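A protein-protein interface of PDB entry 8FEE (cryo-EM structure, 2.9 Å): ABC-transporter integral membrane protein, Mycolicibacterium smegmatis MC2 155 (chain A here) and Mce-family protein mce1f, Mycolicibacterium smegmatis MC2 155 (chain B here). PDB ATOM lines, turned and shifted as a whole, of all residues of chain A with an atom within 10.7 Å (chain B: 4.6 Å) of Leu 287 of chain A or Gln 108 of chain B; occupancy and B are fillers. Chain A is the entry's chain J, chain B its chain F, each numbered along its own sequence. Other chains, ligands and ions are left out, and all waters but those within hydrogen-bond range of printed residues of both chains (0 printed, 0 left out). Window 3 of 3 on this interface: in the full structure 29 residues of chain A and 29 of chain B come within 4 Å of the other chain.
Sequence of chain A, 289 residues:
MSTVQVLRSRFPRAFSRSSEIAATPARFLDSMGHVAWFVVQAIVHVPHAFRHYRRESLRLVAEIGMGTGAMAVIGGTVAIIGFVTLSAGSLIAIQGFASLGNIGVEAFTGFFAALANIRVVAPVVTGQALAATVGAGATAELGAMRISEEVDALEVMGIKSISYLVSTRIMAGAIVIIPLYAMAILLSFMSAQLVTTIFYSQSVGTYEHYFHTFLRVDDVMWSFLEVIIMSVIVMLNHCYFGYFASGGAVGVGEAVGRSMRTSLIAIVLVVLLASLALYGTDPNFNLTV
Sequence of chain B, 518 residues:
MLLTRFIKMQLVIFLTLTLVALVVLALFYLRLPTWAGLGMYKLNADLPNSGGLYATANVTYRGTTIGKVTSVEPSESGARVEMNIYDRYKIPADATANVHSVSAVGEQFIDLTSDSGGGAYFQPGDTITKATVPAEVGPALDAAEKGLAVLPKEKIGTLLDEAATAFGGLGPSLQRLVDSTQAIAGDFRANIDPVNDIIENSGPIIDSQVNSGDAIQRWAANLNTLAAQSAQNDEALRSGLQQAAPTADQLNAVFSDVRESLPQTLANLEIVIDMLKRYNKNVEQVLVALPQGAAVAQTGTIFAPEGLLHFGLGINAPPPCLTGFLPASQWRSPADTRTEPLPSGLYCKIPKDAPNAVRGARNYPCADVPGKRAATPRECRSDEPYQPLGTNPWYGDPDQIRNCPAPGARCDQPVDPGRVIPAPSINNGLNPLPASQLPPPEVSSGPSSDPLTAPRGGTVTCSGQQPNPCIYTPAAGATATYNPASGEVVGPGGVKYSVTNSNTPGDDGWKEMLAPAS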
ATOM      1  N   VAL A 105      -4.425 -35.030  -7.395  1.00  0.00           N
ATOM      2  CA  VAL A 105      -5.622 -34.183  -7.549  1.00  0.00           C
ATOM      3  C   VAL A 105      -5.236 -32.798  -7.040  1.00  0.00           C
ATOM      4  O   VAL A 105      -5.532 -32.396  -5.913  1.00  0.00           O
ATOM      5  CB  VAL A 105      -6.841 -34.775  -6.834  1.00  0.00           C
ATOM      6  CG1 VAL A 105      -7.432 -35.899  -7.661  1.00  0.00           C
ATOM      7  CG2 VAL A 105      -6.450 -35.317  -5.463  1.00  0.00           C
ATOM      8  N   ALA A 107      -5.931 -29.778  -8.771  1.00  0.00           N
ATOM      9  CA  ALA A 107      -6.774 -28.667  -9.192  1.00  0.00           C
ATOM     10  C   ALA A 107      -7.702 -28.190  -8.084  1.00  0.00           C
ATOM     11  O   ALA A 107      -8.260 -27.093  -8.189  1.00  0.00           O
ATOM     12  CB  ALA A 107      -7.597 -29.062 -10.418  1.00  0.00           C
ATOM     13  N   PHE A 108      -7.872 -28.986  -7.028  1.00  0.00           N
ATOM     14  CA  PHE A 108      -8.728 -28.623  -5.907  1.00  0.00           C
ATOM     15  C   PHE A 108      -8.102 -27.591  -4.981  1.00  0.00           C
ATOM     16  O   PHE A 108      -8.825 -27.029  -4.147  1.00  0.00           O
ATOM     17  CB  PHE A 108      -9.083 -29.871  -5.095  1.00  0.00           C
ATOM     18  CG  PHE A 108     -10.048 -30.792  -5.781  1.00  0.00           C
ATOM     19  CD1 PHE A 108     -10.851 -30.336  -6.810  1.00  0.00           C
ATOM     20  CD2 PHE A 108     -10.148 -32.118  -5.398  1.00  0.00           C
ATOM     21  CE1 PHE A 108     -11.741 -31.183  -7.438  1.00  0.00           C
ATOM     22  CE2 PHE A 108     -11.032 -32.969  -6.025  1.00  0.00           C
ATOM     23  CZ  PHE A 108     -11.829 -32.501  -7.045  1.00  0.00           C
ATOM     24  N   PHE A 111     -10.085 -24.322  -4.148  1.00  0.00           N
ATOM     25  CA  PHE A 111     -11.195 -24.502  -3.220  1.00  0.00           C
ATOM     26  C   PHE A 111     -10.662 -24.803  -1.826  1.00  0.00           C
ATOM     27  O   PHE A 111     -11.077 -24.176  -0.842  1.00  0.00           O
ATOM     28  CB  PHE A 111     -12.149 -25.588  -3.741  1.00  0.00           C
ATOM     29  CG  PHE A 111     -12.267 -26.807  -2.857  1.00  0.00           C
ATOM     30  CD1 PHE A 111     -13.157 -26.836  -1.796  1.00  0.00           C
ATOM     31  CD2 PHE A 111     -11.522 -27.942  -3.123  1.00  0.00           C
ATOM     32  CE1 PHE A 111     -13.266 -27.957  -0.999  1.00  0.00           C
ATOM     33  CE2 PHE A 111     -11.630 -29.065  -2.329  1.00  0.00           C
ATOM     34  CZ  PHE A 111     -12.504 -29.073  -1.268  1.00  0.00           C
ATOM     35  N   PHE A 112      -9.675 -25.705  -1.743  1.00  0.00           N
ATOM     36  CA  PHE A 112      -9.071 -26.051  -0.463  1.00  0.00           C
ATOM     37  C   PHE A 112      -8.567 -24.801   0.237  1.00  0.00           C
ATOM     38  O   PHE A 112      -8.865 -24.572   1.416  1.00  0.00           O
ATOM     39  CB  PHE A 112      -7.940 -27.060  -0.675  1.00  0.00           C
ATOM     40  CG  PHE A 112      -7.140 -27.350   0.563  1.00  0.00           C
ATOM     41  CD1 PHE A 112      -7.600 -28.258   1.501  1.00  0.00           C
ATOM     42  CD2 PHE A 112      -5.917 -26.733   0.779  1.00  0.00           C
ATOM     43  CE1 PHE A 112      -6.864 -28.534   2.641  1.00  0.00           C
ATOM     44  CE2 PHE A 112      -5.178 -27.003   1.916  1.00  0.00           C
ATOM     45  CZ  PHE A 112      -5.653 -27.906   2.846  1.00  0.00           C
ATOM     46  N   LEU A 115     -11.299 -22.902   1.914  1.00  0.00           N
ATOM     47  CA  LEU A 115     -11.810 -23.523   3.124  1.00  0.00           C
ATOM     48  C   LEU A 115     -10.758 -23.574   4.217  1.00  0.00           C
ATOM     49  O   LEU A 115     -11.081 -23.929   5.353  1.00  0.00           O
ATOM     50  CB  LEU A 115     -12.345 -24.921   2.814  1.00  0.00           C
ATOM     51  CG  LEU A 115     -13.631 -24.891   1.983  1.00  0.00           C
ATOM     52  CD1 LEU A 115     -14.260 -26.264   1.902  1.00  0.00           C
ATOM     53  CD2 LEU A 115     -14.621 -23.886   2.552  1.00  0.00           C
ATOM     54  N   HIS A 209     -12.098 -20.466 -10.761  1.00  0.00           N
ATOM     55  CA  HIS A 209     -13.345 -21.218 -10.837  1.00  0.00           C
ATOM     56  C   HIS A 209     -13.610 -21.976  -9.545  1.00  0.00           C
ATOM     57  O   HIS A 209     -14.690 -21.858  -8.956  1.00  0.00           O
ATOM     58  CB  HIS A 209     -13.318 -22.188 -12.016  1.00  0.00           C
ATOM     59  CG  HIS A 209     -14.397 -23.225 -11.961  1.00  0.00           C
ATOM     60  ND1 HIS A 209     -15.671 -23.000 -12.437  1.00  0.00           N
ATOM     61  CD2 HIS A 209     -14.395 -24.489 -11.476  1.00  0.00           C
ATOM     62  CE1 HIS A 209     -16.405 -24.082 -12.252  1.00  0.00           C
ATOM     63  NE2 HIS A 209     -15.655 -25.001 -11.670  1.00  0.00           N
ATOM     64  N   TYR A 210     -12.633 -22.766  -9.089  1.00  0.00           N
ATOM     65  CA  TYR A 210     -12.856 -23.564  -7.887  1.00  0.00           C
ATOM     66  C   TYR A 210     -13.044 -22.678  -6.662  1.00  0.00           C
ATOM     67  O   TYR A 210     -13.891 -22.967  -5.806  1.00  0.00           O
ATOM     68  CB  TYR A 210     -11.705 -24.547  -7.685  1.00  0.00           C
ATOM     69  CG  TYR A 210     -11.858 -25.806  -8.506  1.00  0.00           C
ATOM     70  CD1 TYR A 210     -11.416 -25.857  -9.820  1.00  0.00           C
ATOM     71  CD2 TYR A 210     -12.464 -26.935  -7.975  1.00  0.00           C
ATOM     72  CE1 TYR A 210     -11.561 -27.001 -10.578  1.00  0.00           C
ATOM     73  CE2 TYR A 210     -12.614 -28.083  -8.726  1.00  0.00           C
ATOM     74  CZ  TYR A 210     -12.161 -28.111 -10.025  1.00  0.00           C
ATOM     75  OH  TYR A 210     -12.306 -29.254 -10.777  1.00  0.00           O
ATOM     76  N   THR A 213     -16.458 -21.002  -6.821  1.00  0.00           N
ATOM     77  CA  THR A 213     -17.542 -21.972  -6.770  1.00  0.00           C
ATOM     78  C   THR A 213     -17.710 -22.578  -5.382  1.00  0.00           C
ATOM     79  O   THR A 213     -18.842 -22.789  -4.935  1.00  0.00           O
ATOM     80  CB  THR A 213     -17.294 -23.077  -7.803  1.00  0.00           C
ATOM     81  OG1 THR A 213     -17.287 -22.507  -9.118  1.00  0.00           O
ATOM     82  CG2 THR A 213     -18.369 -24.148  -7.732  1.00  0.00           C
ATOM     83  N   PHE A 214     -16.612 -22.831  -4.669  1.00  0.00           N
ATOM     84  CA  PHE A 214     -16.688 -23.508  -3.381  1.00  0.00           C
ATOM     85  C   PHE A 214     -16.480 -22.559  -2.205  1.00  0.00           C
ATOM     86  O   PHE A 214     -16.126 -23.007  -1.109  1.00  0.00           O
ATOM     87  CB  PHE A 214     -15.682 -24.659  -3.325  1.00  0.00           C
ATOM     88  CG  PHE A 214     -15.971 -25.772  -4.299  1.00  0.00           C
ATOM     89  CD1 PHE A 214     -15.732 -25.615  -5.656  1.00  0.00           C
ATOM     90  CD2 PHE A 214     -16.489 -26.975  -3.856  1.00  0.00           C
ATOM     91  CE1 PHE A 214     -16.001 -26.635  -6.545  1.00  0.00           C
ATOM     92  CE2 PHE A 214     -16.761 -27.999  -4.740  1.00  0.00           C
ATOM     93  CZ  PHE A 214     -16.516 -27.827  -6.086  1.00  0.00           C
ATOM     94  N   ARG A 216     -18.509 -19.731   0.131  1.00  0.00           N
ATOM     95  CA  ARG A 216     -19.806 -19.187   0.503  1.00  0.00           C
ATOM     96  C   ARG A 216     -19.609 -17.874   1.246  1.00  0.00           C
ATOM     97  O   ARG A 216     -18.851 -17.815   2.220  1.00  0.00           O
ATOM     98  CB  ARG A 216     -20.594 -20.177   1.365  1.00  0.00           C
ATOM     99  CG  ARG A 216     -21.457 -21.144   0.568  1.00  0.00           C
ATOM    100  CD  ARG A 216     -20.646 -22.293  -0.005  1.00  0.00           C
ATOM    101  NE  ARG A 216     -21.443 -23.124  -0.900  1.00  0.00           N
ATOM    102  CZ  ARG A 216     -22.226 -24.117  -0.503  1.00  0.00           C
ATOM    103  NH1 ARG A 216     -22.342 -24.438   0.774  1.00  0.00           N
ATOM    104  NH2 ARG A 216     -22.911 -24.806  -1.410  1.00  0.00           N
ATOM    105  N   ASP A 282     -24.887 -28.616   9.920  1.00  0.00           N
ATOM    106  CA  ASP A 282     -24.820 -28.375   8.484  1.00  0.00           C
ATOM    107  C   ASP A 282     -23.427 -27.881   8.127  1.00  0.00           C
ATOM    108  O   ASP A 282     -23.076 -26.738   8.459  1.00  0.00           O
ATOM    109  CB  ASP A 282     -25.876 -27.353   8.058  1.00  0.00           C
ATOM    110  CG  ASP A 282     -25.956 -27.192   6.553  1.00  0.00           C
ATOM    111  OD1 ASP A 282     -25.463 -28.084   5.830  1.00  0.00           O
ATOM    112  OD2 ASP A 282     -26.512 -26.173   6.094  1.00  0.00           O
ATOM    113  N   PRO A 283     -22.602 -28.690   7.455  1.00  0.00           N
ATOM    114  CA  PRO A 283     -21.232 -28.256   7.138  1.00  0.00           C
ATOM    115  C   PRO A 283     -21.150 -27.199   6.050  1.00  0.00           C
ATOM    116  O   PRO A 283     -20.053 -26.676   5.817  1.00  0.00           O
ATOM    117  CB  PRO A 283     -20.551 -29.556   6.699  1.00  0.00           C
ATOM    118  CG  PRO A 283     -21.666 -30.393   6.185  1.00  0.00           C
ATOM    119  CD  PRO A 283     -22.858 -30.076   7.034  1.00  0.00           C
ATOM    120  N   ASN A 284     -22.264 -26.876   5.385  1.00  0.00           N
ATOM    121  CA  ASN A 284     -22.322 -25.815   4.375  1.00  0.00           C
ATOM    122  C   ASN A 284     -21.316 -26.056   3.248  1.00  0.00           C
ATOM    123  O   ASN A 284     -20.657 -25.132   2.767  1.00  0.00           O
ATOM    124  CB  ASN A 284     -22.118 -24.438   5.014  1.00  0.00           C
ATOM    125  CG  ASN A 284     -22.605 -23.304   4.131  1.00  0.00           C
ATOM    126  OD1 ASN A 284     -23.461 -23.498   3.268  1.00  0.00           O
ATOM    127  ND2 ASN A 284     -22.059 -22.114   4.343  1.00  0.00           N
ATOM    128  N   PHE A 285     -21.195 -27.313   2.827  1.00  0.00           N
ATOM    129  CA  PHE A 285     -20.281 -27.685   1.753  1.00  0.00           C
ATOM    130  C   PHE A 285     -20.802 -28.945   1.080  1.00  0.00           C
ATOM    131  O   PHE A 285     -21.144 -29.914   1.762  1.00  0.00           O
ATOM    132  CB  PHE A 285     -18.863 -27.905   2.289  1.00  0.00           C
ATOM    133  CG  PHE A 285     -17.929 -28.531   1.296  1.00  0.00           C
ATOM    134  CD1 PHE A 285     -17.511 -27.831   0.179  1.00  0.00           C
ATOM    135  CD2 PHE A 285     -17.463 -29.821   1.486  1.00  0.00           C
ATOM    136  CE1 PHE A 285     -16.654 -28.410  -0.735  1.00  0.00           C
ATOM    137  CE2 PHE A 285     -16.604 -30.405   0.577  1.00  0.00           C
ATOM    138  CZ  PHE A 285     -16.198 -29.698  -0.535  1.00  0.00           C
ATOM    139  N   ASN A 286     -20.872 -28.926  -0.250  1.00  0.00           N
ATOM    140  CA  ASN A 286     -21.401 -30.051  -1.013  1.00  0.00           C
ATOM    141  C   ASN A 286     -20.571 -30.256  -2.271  1.00  0.00           C
ATOM    142  O   ASN A 286     -20.363 -29.313  -3.039  1.00  0.00           O
ATOM    143  CB  ASN A 286     -22.871 -29.824  -1.387  1.00  0.00           C
ATOM    144  CG  ASN A 286     -23.775 -29.743  -0.175  1.00  0.00           C
ATOM    145  OD1 ASN A 286     -24.019 -28.662   0.360  1.00  0.00           O
ATOM    146  ND2 ASN A 286     -24.278 -30.889   0.265  1.00  0.00           N
ATOM    147  N   LEU A 287     -20.097 -31.484  -2.474  1.00  0.00           N
ATOM    148  CA  LEU A 287     -19.420 -31.865  -3.709  1.00  0.00           C
ATOM    149  C   LEU A 287     -20.100 -33.026  -4.415  1.00  0.00           C
ATOM    150  O   LEU A 287     -20.361 -32.944  -5.621  1.00  0.00           O
ATOM    151  CB  LEU A 287     -17.954 -32.220  -3.422  1.00  0.00           C
ATOM    152  CG  LEU A 287     -17.146 -32.702  -4.629  1.00  0.00           C
ATOM    153  CD1 LEU A 287     -16.692 -31.532  -5.488  1.00  0.00           C
ATOM    154  CD2 LEU A 287     -15.963 -33.540  -4.185  1.00  0.00           C
ATOM    155  N   THR A 288     -20.398 -34.107  -3.699  1.00  0.00           N
ATOM    156  CA  THR A 288     -20.946 -35.308  -4.308  1.00  0.00           C
ATOM    157  C   THR A 288     -22.460 -35.176  -4.462  1.00  0.00           C
ATOM    158  O   THR A 288     -23.056 -34.140  -4.153  1.00  0.00           O
ATOM    159  CB  THR A 288     -20.583 -36.538  -3.480  1.00  0.00           C
ATOM    160  OG1 THR A 288     -21.150 -37.707  -4.083  1.00  0.00           O
ATOM    161  CG2 THR A 288     -21.115 -36.398  -2.064  1.00  0.00           C
ATOM    162  N   VAL A 289     -23.096 -36.238  -4.949  1.00  0.00           N
ATOM    163  CA  VAL A 289     -24.539 -36.212  -5.155  1.00  0.00           C
ATOM    164  C   VAL A 289     -25.254 -36.275  -3.810  1.00  0.00           C
ATOM    165  O   VAL A 289     -26.451 -36.003  -3.715  1.00  0.00           O
ATOM    166  CB  VAL A 289     -25.019 -37.360  -6.077  1.00  0.00           C
ATOM    167  CG1 VAL A 289     -24.441 -37.219  -7.474  1.00  0.00           C
ATOM    168  CG2 VAL A 289     -24.692 -38.699  -5.489  1.00  0.00           C
ATOM    169  OXT VAL A 289     -24.657 -36.600  -2.784  1.00  0.00           O
ATOM    170  N   GLY B  51     -30.746 -35.861  -8.962  1.00  0.00           N
ATOM    171  CA  GLY B  51     -29.472 -36.176  -9.569  1.00  0.00           C
ATOM    172  C   GLY B  51     -28.290 -35.687  -8.775  1.00  0.00           C
ATOM    173  O   GLY B  51     -27.179 -35.620  -9.306  1.00  0.00           O
ATOM    174  N   GLY B  52     -28.498 -35.341  -7.507  1.00  0.00           N
ATOM    175  CA  GLY B  52     -27.449 -34.810  -6.671  1.00  0.00           C
ATOM    176  C   GLY B  52     -27.235 -33.317  -6.747  1.00  0.00           C
ATOM    177  O   GLY B  52     -26.312 -32.810  -6.097  1.00  0.00           O
ATOM    178  N   LEU B  53     -28.039 -32.598  -7.529  1.00  0.00           N
ATOM    179  CA  LEU B  53     -27.877 -31.156  -7.635  1.00  0.00           C
ATOM    180  C   LEU B  53     -28.147 -30.492  -6.290  1.00  0.00           C
ATOM    181  O   LEU B  53     -29.058 -30.882  -5.556  1.00  0.00           O
ATOM    182  CB  LEU B  53     -28.821 -30.600  -8.699  1.00  0.00           C
ATOM    183  CG  LEU B  53     -28.538 -29.189  -9.209  1.00  0.00           C
ATOM    184  CD1 LEU B  53     -27.130 -29.107  -9.758  1.00  0.00           C
ATOM    185  CD2 LEU B  53     -29.546 -28.793 -10.270  1.00  0.00           C
ATOM    186  N   TYR B  54     -27.339 -29.486  -5.968  1.00  0.00           N
ATOM    187  CA  TYR B  54     -27.420 -28.780  -4.698  1.00  0.00           C
ATOM    188  C   TYR B  54     -27.496 -27.280  -4.953  1.00  0.00           C
ATOM    189  O   TYR B  54     -27.394 -26.813  -6.090  1.00  0.00           O
ATOM    190  CB  TYR B  54     -26.227 -29.125  -3.792  1.00  0.00           C
ATOM    191  CG  TYR B  54     -24.887 -29.158  -4.498  1.00  0.00           C
ATOM    192  CD1 TYR B  54     -24.243 -27.987  -4.868  1.00  0.00           C
ATOM    193  CD2 TYR B  54     -24.265 -30.363  -4.788  1.00  0.00           C
ATOM    194  CE1 TYR B  54     -23.022 -28.013  -5.509  1.00  0.00           C
ATOM    195  CE2 TYR B  54     -23.043 -30.399  -5.430  1.00  0.00           C
ATOM    196  CZ  TYR B  54     -22.427 -29.220  -5.789  1.00  0.00           C
ATOM    197  OH  TYR B  54     -21.209 -29.247  -6.428  1.00  0.00           O
ATOM    198  N   ALA B  57     -24.675 -24.597  -6.864  1.00  0.00           N
ATOM    199  CA  ALA B  57     -24.114 -25.251  -8.036  1.00  0.00           C
ATOM    200  C   ALA B  57     -24.303 -24.380  -9.272  1.00  0.00           C
ATOM    201  O   ALA B  57     -25.290 -23.654  -9.403  1.00  0.00           O
ATOM    202  CB  ALA B  57     -24.769 -26.613  -8.254  1.00  0.00           C
ATOM    203  N   HIS B 100     -25.682 -32.589 -14.711  1.00  0.00           N
ATOM    204  CA  HIS B 100     -24.424 -33.195 -15.114  1.00  0.00           C
ATOM    205  C   HIS B 100     -23.465 -33.233 -13.934  1.00  0.00           C
ATOM    206  O   HIS B 100     -23.622 -32.502 -12.953  1.00  0.00           O
ATOM    207  CB  HIS B 100     -23.787 -32.442 -16.286  1.00  0.00           C
ATOM    208  CG  HIS B 100     -24.402 -32.756 -17.614  1.00  0.00           C
ATOM    209  ND1 HIS B 100     -24.979 -33.974 -17.896  1.00  0.00           N
ATOM    210  CD2 HIS B 100     -24.530 -32.010 -18.736  1.00  0.00           C
ATOM    211  CE1 HIS B 100     -25.436 -33.965 -19.136  1.00  0.00           C
ATOM    212  NE2 HIS B 100     -25.176 -32.785 -19.668  1.00  0.00           N
ATOM    213  N   SER B 101     -22.463 -34.101 -14.043  1.00  0.00           N
ATOM    214  CA  SER B 101     -21.376 -34.193 -13.079  1.00  0.00           C
ATOM    215  C   SER B 101     -20.059 -33.966 -13.807  1.00  0.00           C
ATOM    216  O   SER B 101     -19.828 -34.554 -14.869  1.00  0.00           O
ATOM    217  CB  SER B 101     -21.377 -35.553 -12.377  1.00  0.00           C
ATOM    218  OG  SER B 101     -20.421 -35.595 -11.335  1.00  0.00           O
ATOM    219  N   VAL B 105     -15.592 -37.579  -9.042  1.00  0.00           N
ATOM    220  CA  VAL B 105     -15.595 -37.289  -7.614  1.00  0.00           C
ATOM    221  C   VAL B 105     -16.778 -36.421  -7.191  1.00  0.00           C
ATOM    222  O   VAL B 105     -17.136 -36.424  -6.004  1.00  0.00           O
ATOM    223  CB  VAL B 105     -14.271 -36.626  -7.181  1.00  0.00           C
ATOM    224  CG1 VAL B 105     -13.133 -37.630  -7.240  1.00  0.00           C
ATOM    225  CG2 VAL B 105     -13.970 -35.424  -8.057  1.00  0.00           C
ATOM    226  N   GLY B 106     -17.390 -35.686  -8.116  1.00  0.00           N
ATOM    227  CA  GLY B 106     -18.569 -34.906  -7.802  1.00  0.00           C
ATOM    228  C   GLY B 106     -18.687 -33.641  -8.627  1.00  0.00           C
ATOM    229  O   GLY B 106     -18.498 -33.672  -9.846  1.00  0.00           O
ATOM    230  N   GLU B 107     -19.012 -32.528  -7.963  1.00  0.00           N
ATOM    231  CA  GLU B 107     -19.223 -31.223  -8.593  1.00  0.00           C
ATOM    232  C   GLU B 107     -20.359 -31.293  -9.619  1.00  0.00           C
ATOM    233  O   GLU B 107     -20.164 -31.206 -10.832  1.00  0.00           O
ATOM    234  CB  GLU B 107     -17.928 -30.689  -9.221  1.00  0.00           C
ATOM    235  CG  GLU B 107     -18.005 -29.235  -9.662  1.00  0.00           C
ATOM    236  CD  GLU B 107     -16.715 -28.742 -10.276  1.00  0.00           C
ATOM    237  OE1 GLU B 107     -15.706 -29.474 -10.206  1.00  0.00           O
ATOM    238  OE2 GLU B 107     -16.708 -27.623 -10.830  1.00  0.00           O
ATOM    239  N   GLN B 108     -21.562 -31.488  -9.088  1.00  0.00           N
ATOM    240  CA  GLN B 108     -22.753 -31.462  -9.921  1.00  0.00           C
ATOM    241  C   GLN B 108     -23.019 -30.047 -10.422  1.00  0.00           C
ATOM    242  O   GLN B 108     -22.590 -29.055  -9.827  1.00  0.00           O
ATOM    243  CB  GLN B 108     -23.961 -31.974  -9.140  1.00  0.00           C
ATOM    244  CG  GLN B 108     -23.610 -33.028  -8.115  1.00  0.00           C
ATOM    245  CD  GLN B 108     -23.071 -34.290  -8.742  1.00  0.00           C
ATOM    246  OE1 GLN B 108     -23.465 -34.667  -9.844  1.00  0.00           O
ATOM    247  NE2 GLN B 108     -22.143 -34.940  -8.051  1.00  0.00           N
ATOM    248  N   PHE B 109     -23.745 -29.965 -11.530  1.00  0.00           N
ATOM    249  CA  PHE B 109     -24.226 -28.692 -12.053  1.00  0.00           C
ATOM    250  C   PHE B 109     -25.382 -28.979 -13.002  1.00  0.00           C
ATOM    251  O   PHE B 109     -25.761 -30.132 -13.216  1.00  0.00           O
ATOM    252  CB  PHE B 109     -23.109 -27.901 -12.743  1.00  0.00           C
ATOM    253  CG  PHE B 109     -22.601 -28.531 -14.007  1.00  0.00           C
ATOM    254  CD1 PHE B 109     -21.760 -29.629 -13.967  1.00  0.00           C
ATOM    255  CD2 PHE B 109     -22.959 -28.015 -15.241  1.00  0.00           C
ATOM    256  CE1 PHE B 109     -21.293 -30.202 -15.131  1.00  0.00           C
ATOM    257  CE2 PHE B 109     -22.495 -28.586 -16.406  1.00  0.00           C
ATOM    258  CZ  PHE B 109     -21.661 -29.678 -16.351  1.00  0.00           C
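The side-chain hydroxyl (OH) of Tyr 54 of chain B sits close to the backbone carbonyl oxygen (O) of Asn 286 of chain A, 3.5 Å away.
OE2 of Glu 107 of chain B lies within hydrogen-bond range of NE2 of His 209 of chain A (2.9 Å).
The side-chain carboxylate of Glu 107 of chain B is in hydrogen-bond range of the side-chain hydroxyl of Tyr 210 of chain A (3.5 Å).
O of Leu 287 of chain A sits at hydrogen-bond distance from N of Glu 107 of chain B (2.7 Å).
The side-chain amide nitrogen (NE2) of Gln 108 of chain B lies close to the backbone NH (N) of Val 289 of chain A.
OH of Tyr 54 of chain B is in hydrogen-bond range of N of Gln 108 of chain B (3.5 Å).
O of Gly 106 of chain B lies within hydrogen-bond range of OG of Ser 101 of chain B (3.1 Å).
The side-chain hydroxyl (OG1) of Thr 213 of chain A sits at hydrogen-bond distance from the backbone carbonyl oxygen (O) of His 209 of chain A (2.7 Å).
Phe 108 of chain A touches Val 105 of chain B (CZ to CG2, 3.8 Å).
CE2 of Tyr 54 of chain B touches O of Leu 287 of chain A, at 3.7 Å.
Leu 287 of chain A touches Val 105 of chain B.
Leu 287 of chain A touches Gly 106 of chain B (O to CA, 3.4 Å).
Leu 287 of chain A touches Gln 108 of chain B (O to NE2, 3.6 Å).
Tyr 54 of chain B touches Thr 288 of chain A.
C of Thr 288 of chain A touches NE2 of Gln 108 of chain B, at 3.6 Å.
Val 289 of chain A touches Gly 51 of chain B (CG1 to O, 3.7 Å).
Gly 52 of chain B touches Val 289 of chain A.
Of chain B, only Tyr 54 (3.7 Å), Val 105 (3.6 Å), Gly 106 (3.4 Å), Glu 107 (2.7 Å) and Gln 108 (3.6 Å) come within 4 Å of Leu 287 of chain A.
Gln 108 of chain B touches three residues of chain A.
No residue of chain A comes within 4 Å of Leu 53 of chain B.
Of chain A, only Phe 108 (3.8 Å) and Leu 287 (3.6 Å) come within 4 Å of Val 105 of chain B.
No residue of chain A comes within 4 Å of Phe 109 of chain B.
Of the printed residues of chain B, Val 289 of chain A touches Gly 51 (3.7 Å), Gly 52 (3.3 Å) and Gln 108 (3.3 Å).
Of the printed residues of chain B, Asn 286 of chain A touches Tyr 54 (3.4 Å).
Printed residues of chain B within 4 Å of Tyr 210 of chain A: Glu 107.
Of the printed residues of chain B, His 209 of chain A touches Glu 107 (2.9 Å).
Printed residues of chain A within 4 Å of Gly 51 of chain B: Val 289.
The nearest printed residue of chain B that does not touch Leu 287 of chain A is Gly 52 of chain B (6.0 Å).
The nearest printed residue of chain B that does not touch Val 289 of chain A is Leu 53 of chain B (5.4 Å).
Of the 19 printed residues of chain A, 7 touch a printed residue of chain B.
Printed residues of chain A that touch a printed residue of chain B: Phe 108, His 209, Tyr 210, Asn 286, Leu 287, Thr 288 and Val 289.
Among the printed residues, 14 pairs touch across the chains.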
